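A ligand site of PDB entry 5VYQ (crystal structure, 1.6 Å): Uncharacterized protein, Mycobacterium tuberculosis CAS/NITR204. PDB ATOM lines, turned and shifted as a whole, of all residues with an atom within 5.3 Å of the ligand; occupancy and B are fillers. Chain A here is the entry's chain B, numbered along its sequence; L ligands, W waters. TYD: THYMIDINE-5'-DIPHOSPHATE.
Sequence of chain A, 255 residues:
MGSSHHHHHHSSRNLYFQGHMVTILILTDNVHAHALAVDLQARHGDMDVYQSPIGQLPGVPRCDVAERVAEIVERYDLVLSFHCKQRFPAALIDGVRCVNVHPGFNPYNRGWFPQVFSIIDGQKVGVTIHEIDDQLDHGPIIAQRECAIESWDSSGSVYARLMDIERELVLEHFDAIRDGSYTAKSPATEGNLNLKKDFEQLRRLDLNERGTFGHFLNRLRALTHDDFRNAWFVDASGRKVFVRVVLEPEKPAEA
The side-chain amino group (NZ) of Lys 85 lies within salt-bridge range of an oxygen (O2B) of the ligand, at 2.5 Å.
OH of Tyr 159 lies within hydrogen-bond range of O3B of the ligand.
O3' of the ligand is in hydrogen-bond range of NE2 of Gln 115.
An oxygen (O2) of the ligand is in hydrogen-bond range of the side-chain amide nitrogen (ND2) of Asn 230, 2.9 Å away.
A ring nitrogen (ND1) of His 83 sits at hydrogen-bond distance from an oxygen (O1B) of the ligand (2.9 Å).
The side-chain amide nitrogen (ND2) of Asn 30 sits at hydrogen-bond distance from an oxygen (O1B) of the ligand (2.9 Å).
A ring nitrogen (NE2) of His 225 is in hydrogen-bond range of an oxygen (O4') of the ligand, at 3.4 Å.
The side-chain amino group of Lys 85 sits at hydrogen-bond distance from the backbone carbonyl oxygen of His 83, at 3.0 Å.
The side-chain hydroxyl (OH) of Tyr 159 is in hydrogen-bond range of the side-chain amide nitrogen (ND2) of Asn 30 (2.8 Å).
NE2 of Gln 115 sits at hydrogen-bond distance from OG of Ser 155, at 2.9 Å.
A ring nitrogen (ND1) of His 83 is in hydrogen-bond range of the side-chain amide nitrogen (ND2) of Asn 30.
ND1 of His 225 is in hydrogen-bond range of OG of Ser 155, at 2.8 Å.
Phe 113 touches the ligand (CD1 to C3', 3.4 Å).
Phe 199 touches the ligand (CZ to N3, 3.9 Å).
Phe 228 touches the ligand.
Hydrophobic or aromatic side chains within 4 Å of the ligand: His 83, Phe 113, Tyr 159, Phe 199, His 225 and Phe 228.
Water W8 lies within hydrogen-bond range of an oxygen (O2B) of the ligand (2.6 Å) and the backbone NH (N) of Phe 113 (3.0 Å).
Water W1 lies within hydrogen-bond range of OD1 of Asn 230 and O4 of the ligand.
Water W6 lies within hydrogen-bond range of the backbone NH of Val 31 (2.8 Å) and an oxygen (O2A) of the ligand (3.1 Å).
Water W3 lies within hydrogen-bond range of the side-chain amide nitrogen of Asn 230 (3.0 Å), an oxygen (O2) of the ligand (3.3 Å) and the side-chain hydroxyl of Ser 155 (3.5 Å).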
ATOM      1  N   ASN A  30      30.690  31.589 -29.413  1.00  0.00           N
ATOM      2  CA  ASN A  30      29.567  30.892 -28.838  1.00  0.00           C
ATOM      3  C   ASN A  30      28.396  30.934 -29.776  1.00  0.00           C
ATOM      4  O   ASN A  30      28.023  31.995 -30.313  1.00  0.00           O
ATOM      5  CB  ASN A  30      29.212  31.553 -27.531  1.00  0.00           C
ATOM      6  CG  ASN A  30      28.012  30.938 -26.878  1.00  0.00           C
ATOM      7  OD1 ASN A  30      26.891  31.372 -27.145  1.00  0.00           O
ATOM      8  ND2 ASN A  30      28.222  29.946 -26.014  1.00  0.00           N
ATOM      9  N   VAL A  31      27.765  29.781 -29.961  1.00  0.00           N
ATOM     10  CA  VAL A  31      26.612  29.718 -30.860  1.00  0.00           C
ATOM     11  C   VAL A  31      25.418  30.588 -30.499  1.00  0.00           C
ATOM     12  O   VAL A  31      24.809  31.218 -31.381  1.00  0.00           O
ATOM     13  CB  VAL A  31      26.185  28.237 -31.086  1.00  0.00           C
ATOM     14  CG1 VAL A  31      25.710  27.637 -29.783  1.00  0.00           C
ATOM     15  CG2 VAL A  31      25.097  28.176 -32.137  1.00  0.00           C
ATOM     16  N   HIS A  83      31.641  36.062 -24.154  1.00  0.00           N
ATOM     17  CA  HIS A  83      32.208  34.852 -23.540  1.00  0.00           C
ATOM     18  C   HIS A  83      33.709  34.729 -23.830  1.00  0.00           C
ATOM     19  O   HIS A  83      34.239  33.628 -23.972  1.00  0.00           O
ATOM     20  CB  HIS A  83      31.494  33.563 -23.957  1.00  0.00           C
ATOM     21  CG  HIS A  83      29.996  33.579 -23.875  1.00  0.00           C
ATOM     22  ND1 HIS A  83      29.267  32.412 -23.977  1.00  0.00           N
ATOM     23  CD2 HIS A  83      29.096  34.573 -23.707  1.00  0.00           C
ATOM     24  CE1 HIS A  83      27.975  32.684 -23.851  1.00  0.00           C
ATOM     25  NE2 HIS A  83      27.851  33.993 -23.656  1.00  0.00           N
ATOM     26  N   LYS A  85      37.575  34.409 -23.498  1.00  0.00           N
ATOM     27  CA  LYS A  85      38.355  33.631 -22.563  1.00  0.00           C
ATOM     28  C   LYS A  85      39.752  34.163 -22.338  1.00  0.00           C
ATOM     29  O   LYS A  85      40.377  33.713 -21.383  1.00  0.00           O
ATOM     30  CB  LYS A  85      38.562  32.190 -23.038  1.00  0.00           C
ATOM     31  CG  LYS A  85      37.293  31.401 -23.284  1.00  0.00           C
ATOM     32  CD  LYS A  85      36.446  31.323 -22.017  1.00  0.00           C
ATOM     33  CE  LYS A  85      35.262  30.376 -22.153  1.00  0.00           C
ATOM     34  NZ  LYS A  85      34.283  30.721 -23.214  1.00  0.00           N
ATOM     35  N   PRO A 103      29.066  35.219 -19.169  1.00  0.00           N
ATOM     36  CA  PRO A 103      27.925  34.499 -18.623  1.00  0.00           C
ATOM     37  C   PRO A 103      28.226  33.962 -17.220  1.00  0.00           C
ATOM     38  O   PRO A 103      27.953  32.800 -16.905  1.00  0.00           O
ATOM     39  CB  PRO A 103      27.711  33.430 -19.691  1.00  0.00           C
ATOM     40  CG  PRO A 103      29.076  33.016 -20.078  1.00  0.00           C
ATOM     41  CD  PRO A 103      29.815  34.366 -20.109  1.00  0.00           C
ATOM     42  N   PHE A 113      32.989  28.573 -17.651  1.00  0.00           N
ATOM     43  CA  PHE A 113      31.743  27.852 -17.349  1.00  0.00           C
ATOM     44  C   PHE A 113      31.213  28.152 -15.946  1.00  0.00           C
ATOM     45  O   PHE A 113      31.087  27.270 -15.061  1.00  0.00           O
ATOM     46  CB  PHE A 113      32.005  26.336 -17.428  1.00  0.00           C
ATOM     47  CG  PHE A 113      32.544  25.873 -18.773  1.00  0.00           C
ATOM     48  CD1 PHE A 113      32.494  26.652 -19.927  1.00  0.00           C
ATOM     49  CD2 PHE A 113      33.051  24.619 -18.878  1.00  0.00           C
ATOM     50  CE1 PHE A 113      32.982  26.171 -21.128  1.00  0.00           C
ATOM     51  CE2 PHE A 113      33.562  24.118 -20.068  1.00  0.00           C
ATOM     52  CZ  PHE A 113      33.512  24.906 -21.201  1.00  0.00           C
ATOM     53  N   GLN A 115      28.391  28.609 -14.304  1.00  0.00           N
ATOM     54  CA  GLN A 115      27.310  27.873 -13.654  1.00  0.00           C
ATOM     55  C   GLN A 115      27.814  26.504 -13.177  1.00  0.00           C
ATOM     56  O   GLN A 115      27.240  26.019 -12.212  1.00  0.00           O
ATOM     57  CB  GLN A 115      26.068  27.726 -14.544  1.00  0.00           C
ATOM     58  CG  GLN A 115      26.151  26.686 -15.643  1.00  0.00           C
ATOM     59  CD  GLN A 115      27.067  27.105 -16.787  1.00  0.00           C
ATOM     60  OE1 GLN A 115      27.511  28.253 -16.874  1.00  0.00           O
ATOM     61  NE2 GLN A 115      27.368  26.154 -17.658  1.00  0.00           N
ATOM     62  N   VAL A 116      28.782  25.875 -13.812  1.00  0.00           N
ATOM     63  CA  VAL A 116      29.349  24.635 -13.268  1.00  0.00           C
ATOM     64  C   VAL A 116      29.861  24.829 -11.847  1.00  0.00           C
ATOM     65  O   VAL A 116      29.540  24.123 -10.871  1.00  0.00           O
ATOM     66  CB  VAL A 116      30.449  24.111 -14.209  1.00  0.00           C
ATOM     67  CG1 VAL A 116      31.132  22.907 -13.555  1.00  0.00           C
ATOM     68  CG2 VAL A 116      29.867  23.768 -15.589  1.00  0.00           C
ATOM     69  N   SER A 155      24.051  21.937 -15.141  1.00  0.00           N
ATOM     70  CA  SER A 155      24.745  22.952 -15.943  1.00  0.00           C
ATOM     71  C   SER A 155      23.897  23.293 -17.151  1.00  0.00           C
ATOM     72  O   SER A 155      23.714  24.484 -17.465  1.00  0.00           O
ATOM     73  CB  SER A 155      26.151  22.477 -16.303  1.00  0.00           C
ATOM     74  OG  SER A 155      26.717  23.335 -17.282  1.00  0.00           O
ATOM     75  N   TYR A 159      22.374  26.989 -17.880  1.00  0.00           N
ATOM     76  CA  TYR A 159      22.912  27.656 -19.091  1.00  0.00           C
ATOM     77  C   TYR A 159      21.849  28.128 -20.086  1.00  0.00           C
ATOM     78  O   TYR A 159      21.935  29.242 -20.637  1.00  0.00           O
ATOM     79  CB  TYR A 159      23.916  26.722 -19.729  1.00  0.00           C
ATOM     80  CG  TYR A 159      24.687  27.350 -20.831  1.00  0.00           C
ATOM     81  CD1 TYR A 159      25.728  28.208 -20.514  1.00  0.00           C
ATOM     82  CD2 TYR A 159      24.387  27.111 -22.174  1.00  0.00           C
ATOM     83  CE1 TYR A 159      26.502  28.803 -21.478  1.00  0.00           C
ATOM     84  CE2 TYR A 159      25.163  27.758 -23.154  1.00  0.00           C
ATOM     85  CZ  TYR A 159      26.186  28.609 -22.756  1.00  0.00           C
ATOM     86  OH  TYR A 159      27.123  29.284 -23.534  1.00  0.00           O
ATOM     87  N   PHE A 199      38.049  23.045 -14.692  1.00  0.00           N
ATOM     88  CA  PHE A 199      36.905  22.266 -15.170  1.00  0.00           C
ATOM     89  C   PHE A 199      37.353  20.854 -15.466  1.00  0.00           C
ATOM     90  O   PHE A 199      36.714  19.855 -15.076  1.00  0.00           O
ATOM     91  CB  PHE A 199      36.318  22.868 -16.440  1.00  0.00           C
ATOM     92  CG  PHE A 199      35.201  22.041 -17.030  1.00  0.00           C
ATOM     93  CD1 PHE A 199      33.952  22.060 -16.433  1.00  0.00           C
ATOM     94  CD2 PHE A 199      35.382  21.241 -18.140  1.00  0.00           C
ATOM     95  CE1 PHE A 199      32.889  21.332 -16.949  1.00  0.00           C
ATOM     96  CE2 PHE A 199      34.335  20.520 -18.669  1.00  0.00           C
ATOM     97  CZ  PHE A 199      33.096  20.548 -18.062  1.00  0.00           C
ATOM     98  N   HIS A 225      25.359  18.394 -18.773  1.00  0.00           N
ATOM     99  CA  HIS A 225      25.104  19.464 -19.732  1.00  0.00           C
ATOM    100  C   HIS A 225      24.744  18.819 -21.087  1.00  0.00           C
ATOM    101  O   HIS A 225      25.625  18.458 -21.854  1.00  0.00           O
ATOM    102  CB  HIS A 225      26.321  20.386 -19.846  1.00  0.00           C
ATOM    103  CG  HIS A 225      26.009  21.664 -20.566  1.00  0.00           C
ATOM    104  ND1 HIS A 225      26.042  22.889 -19.928  1.00  0.00           N
ATOM    105  CD2 HIS A 225      25.583  21.900 -21.822  1.00  0.00           C
ATOM    106  CE1 HIS A 225      25.700  23.825 -20.783  1.00  0.00           C
ATOM    107  NE2 HIS A 225      25.415  23.247 -21.947  1.00  0.00           N
ATOM    108  N   PHE A 228      26.907  16.129 -23.344  1.00  0.00           N
ATOM    109  CA  PHE A 228      28.342  16.115 -23.058  1.00  0.00           C
ATOM    110  C   PHE A 228      28.748  14.982 -22.097  1.00  0.00           C
ATOM    111  O   PHE A 228      28.124  14.732 -21.048  1.00  0.00           O
ATOM    112  CB  PHE A 228      28.834  17.422 -22.432  1.00  0.00           C
ATOM    113  CG  PHE A 228      29.112  18.534 -23.395  1.00  0.00           C
ATOM    114  CD1 PHE A 228      30.209  18.454 -24.243  1.00  0.00           C
ATOM    115  CD2 PHE A 228      28.325  19.651 -23.434  1.00  0.00           C
ATOM    116  CE1 PHE A 228      30.488  19.486 -25.113  1.00  0.00           C
ATOM    117  CE2 PHE A 228      28.579  20.684 -24.326  1.00  0.00           C
ATOM    118  CZ  PHE A 228      29.664  20.590 -25.169  1.00  0.00           C
ATOM    119  N   ASN A 230      30.981  14.677 -19.822  1.00  0.00           N
ATOM    120  CA  ASN A 230      31.903  15.352 -18.938  1.00  0.00           C
ATOM    121  C   ASN A 230      32.480  14.476 -17.811  1.00  0.00           C
ATOM    122  O   ASN A 230      33.681  14.353 -17.702  1.00  0.00           O
ATOM    123  CB  ASN A 230      31.275  16.624 -18.325  1.00  0.00           C
ATOM    124  CG  ASN A 230      30.945  17.699 -19.344  1.00  0.00           C
ATOM    125  OD1 ASN A 230      31.669  17.988 -20.346  1.00  0.00           O
ATOM    126  ND2 ASN A 230      29.836  18.386 -19.071  1.00  0.00           N
HETATM  127  PA  TYD L   1      30.806  26.833 -24.801  1.00  0.00           P
HETATM  128  O1A TYD L   1      32.088  26.081 -25.130  1.00  0.00           O
HETATM  129  O2A TYD L   1      29.865  27.394 -25.822  1.00  0.00           O
HETATM  130  O3A TYD L   1      31.209  27.883 -23.643  1.00  0.00           O
HETATM  131  PB  TYD L   1      30.843  29.386 -23.392  1.00  0.00           P
HETATM  132  O1B TYD L   1      30.853  30.092 -24.746  1.00  0.00           O
HETATM  133  O2B TYD L   1      32.097  29.670 -22.569  1.00  0.00           O
HETATM  134  O3B TYD L   1      29.594  29.584 -22.591  1.00  0.00           O
HETATM  135  O5' TYD L   1      30.013  25.941 -23.706  1.00  0.00           O
HETATM  136  C5' TYD L   1      28.791  26.484 -23.208  1.00  0.00           C
HETATM  137  C4' TYD L   1      28.513  25.510 -22.102  1.00  0.00           C
HETATM  138  O4' TYD L   1      28.625  24.136 -22.574  1.00  0.00           O
HETATM  139  C3' TYD L   1      29.428  25.644 -20.907  1.00  0.00           C
HETATM  140  O3' TYD L   1      28.984  26.637 -19.964  1.00  0.00           O
HETATM  141  C2' TYD L   1      29.404  24.236 -20.346  1.00  0.00           C
HETATM  142  C1' TYD L   1      29.041  23.322 -21.506  1.00  0.00           C
HETATM  143  N1  TYD L   1      30.215  22.519 -21.929  1.00  0.00           N
HETATM  144  C2  TYD L   1      30.419  21.308 -21.307  1.00  0.00           C
HETATM  145  O2  TYD L   1      29.642  20.934 -20.418  1.00  0.00           O
HETATM  146  N3  TYD L   1      31.470  20.556 -21.658  1.00  0.00           N
HETATM  147  C4  TYD L   1      32.342  20.928 -22.604  1.00  0.00           C
HETATM  148  O4  TYD L   1      33.318  20.187 -22.897  1.00  0.00           O
HETATM  149  C5  TYD L   1      32.157  22.247 -23.240  1.00  0.00           C
HETATM  150  C5M TYD L   1      33.114  22.737 -24.331  1.00  0.00           C
HETATM  151  C6  TYD L   1      31.046  22.990 -22.878  1.00  0.00           C
HETATM  152  O   HOH W   1      33.831  17.474 -21.804  1.00  0.00           O
HETATM  153  O   HOH W   2      32.155  24.802 -27.460  1.00  0.00           O
HETATM  154  O   HOH W   3      28.810  20.546 -17.275  1.00  0.00           O
HETATM  155  O   HOH W   4      34.226  19.528 -25.510  1.00  0.00           O
HETATM  156  O   HOH W   5      34.522  26.643 -24.689  1.00  0.00           O
HETATM  157  O   HOH W   6      28.880  27.502 -28.763  1.00  0.00           O
HETATM  158  O   HOH W   7      29.677  29.199 -20.084  1.00  0.00           O
HETATM  159  O   HOH W   8      32.360  30.215 -20.071  1.00  0.00           O
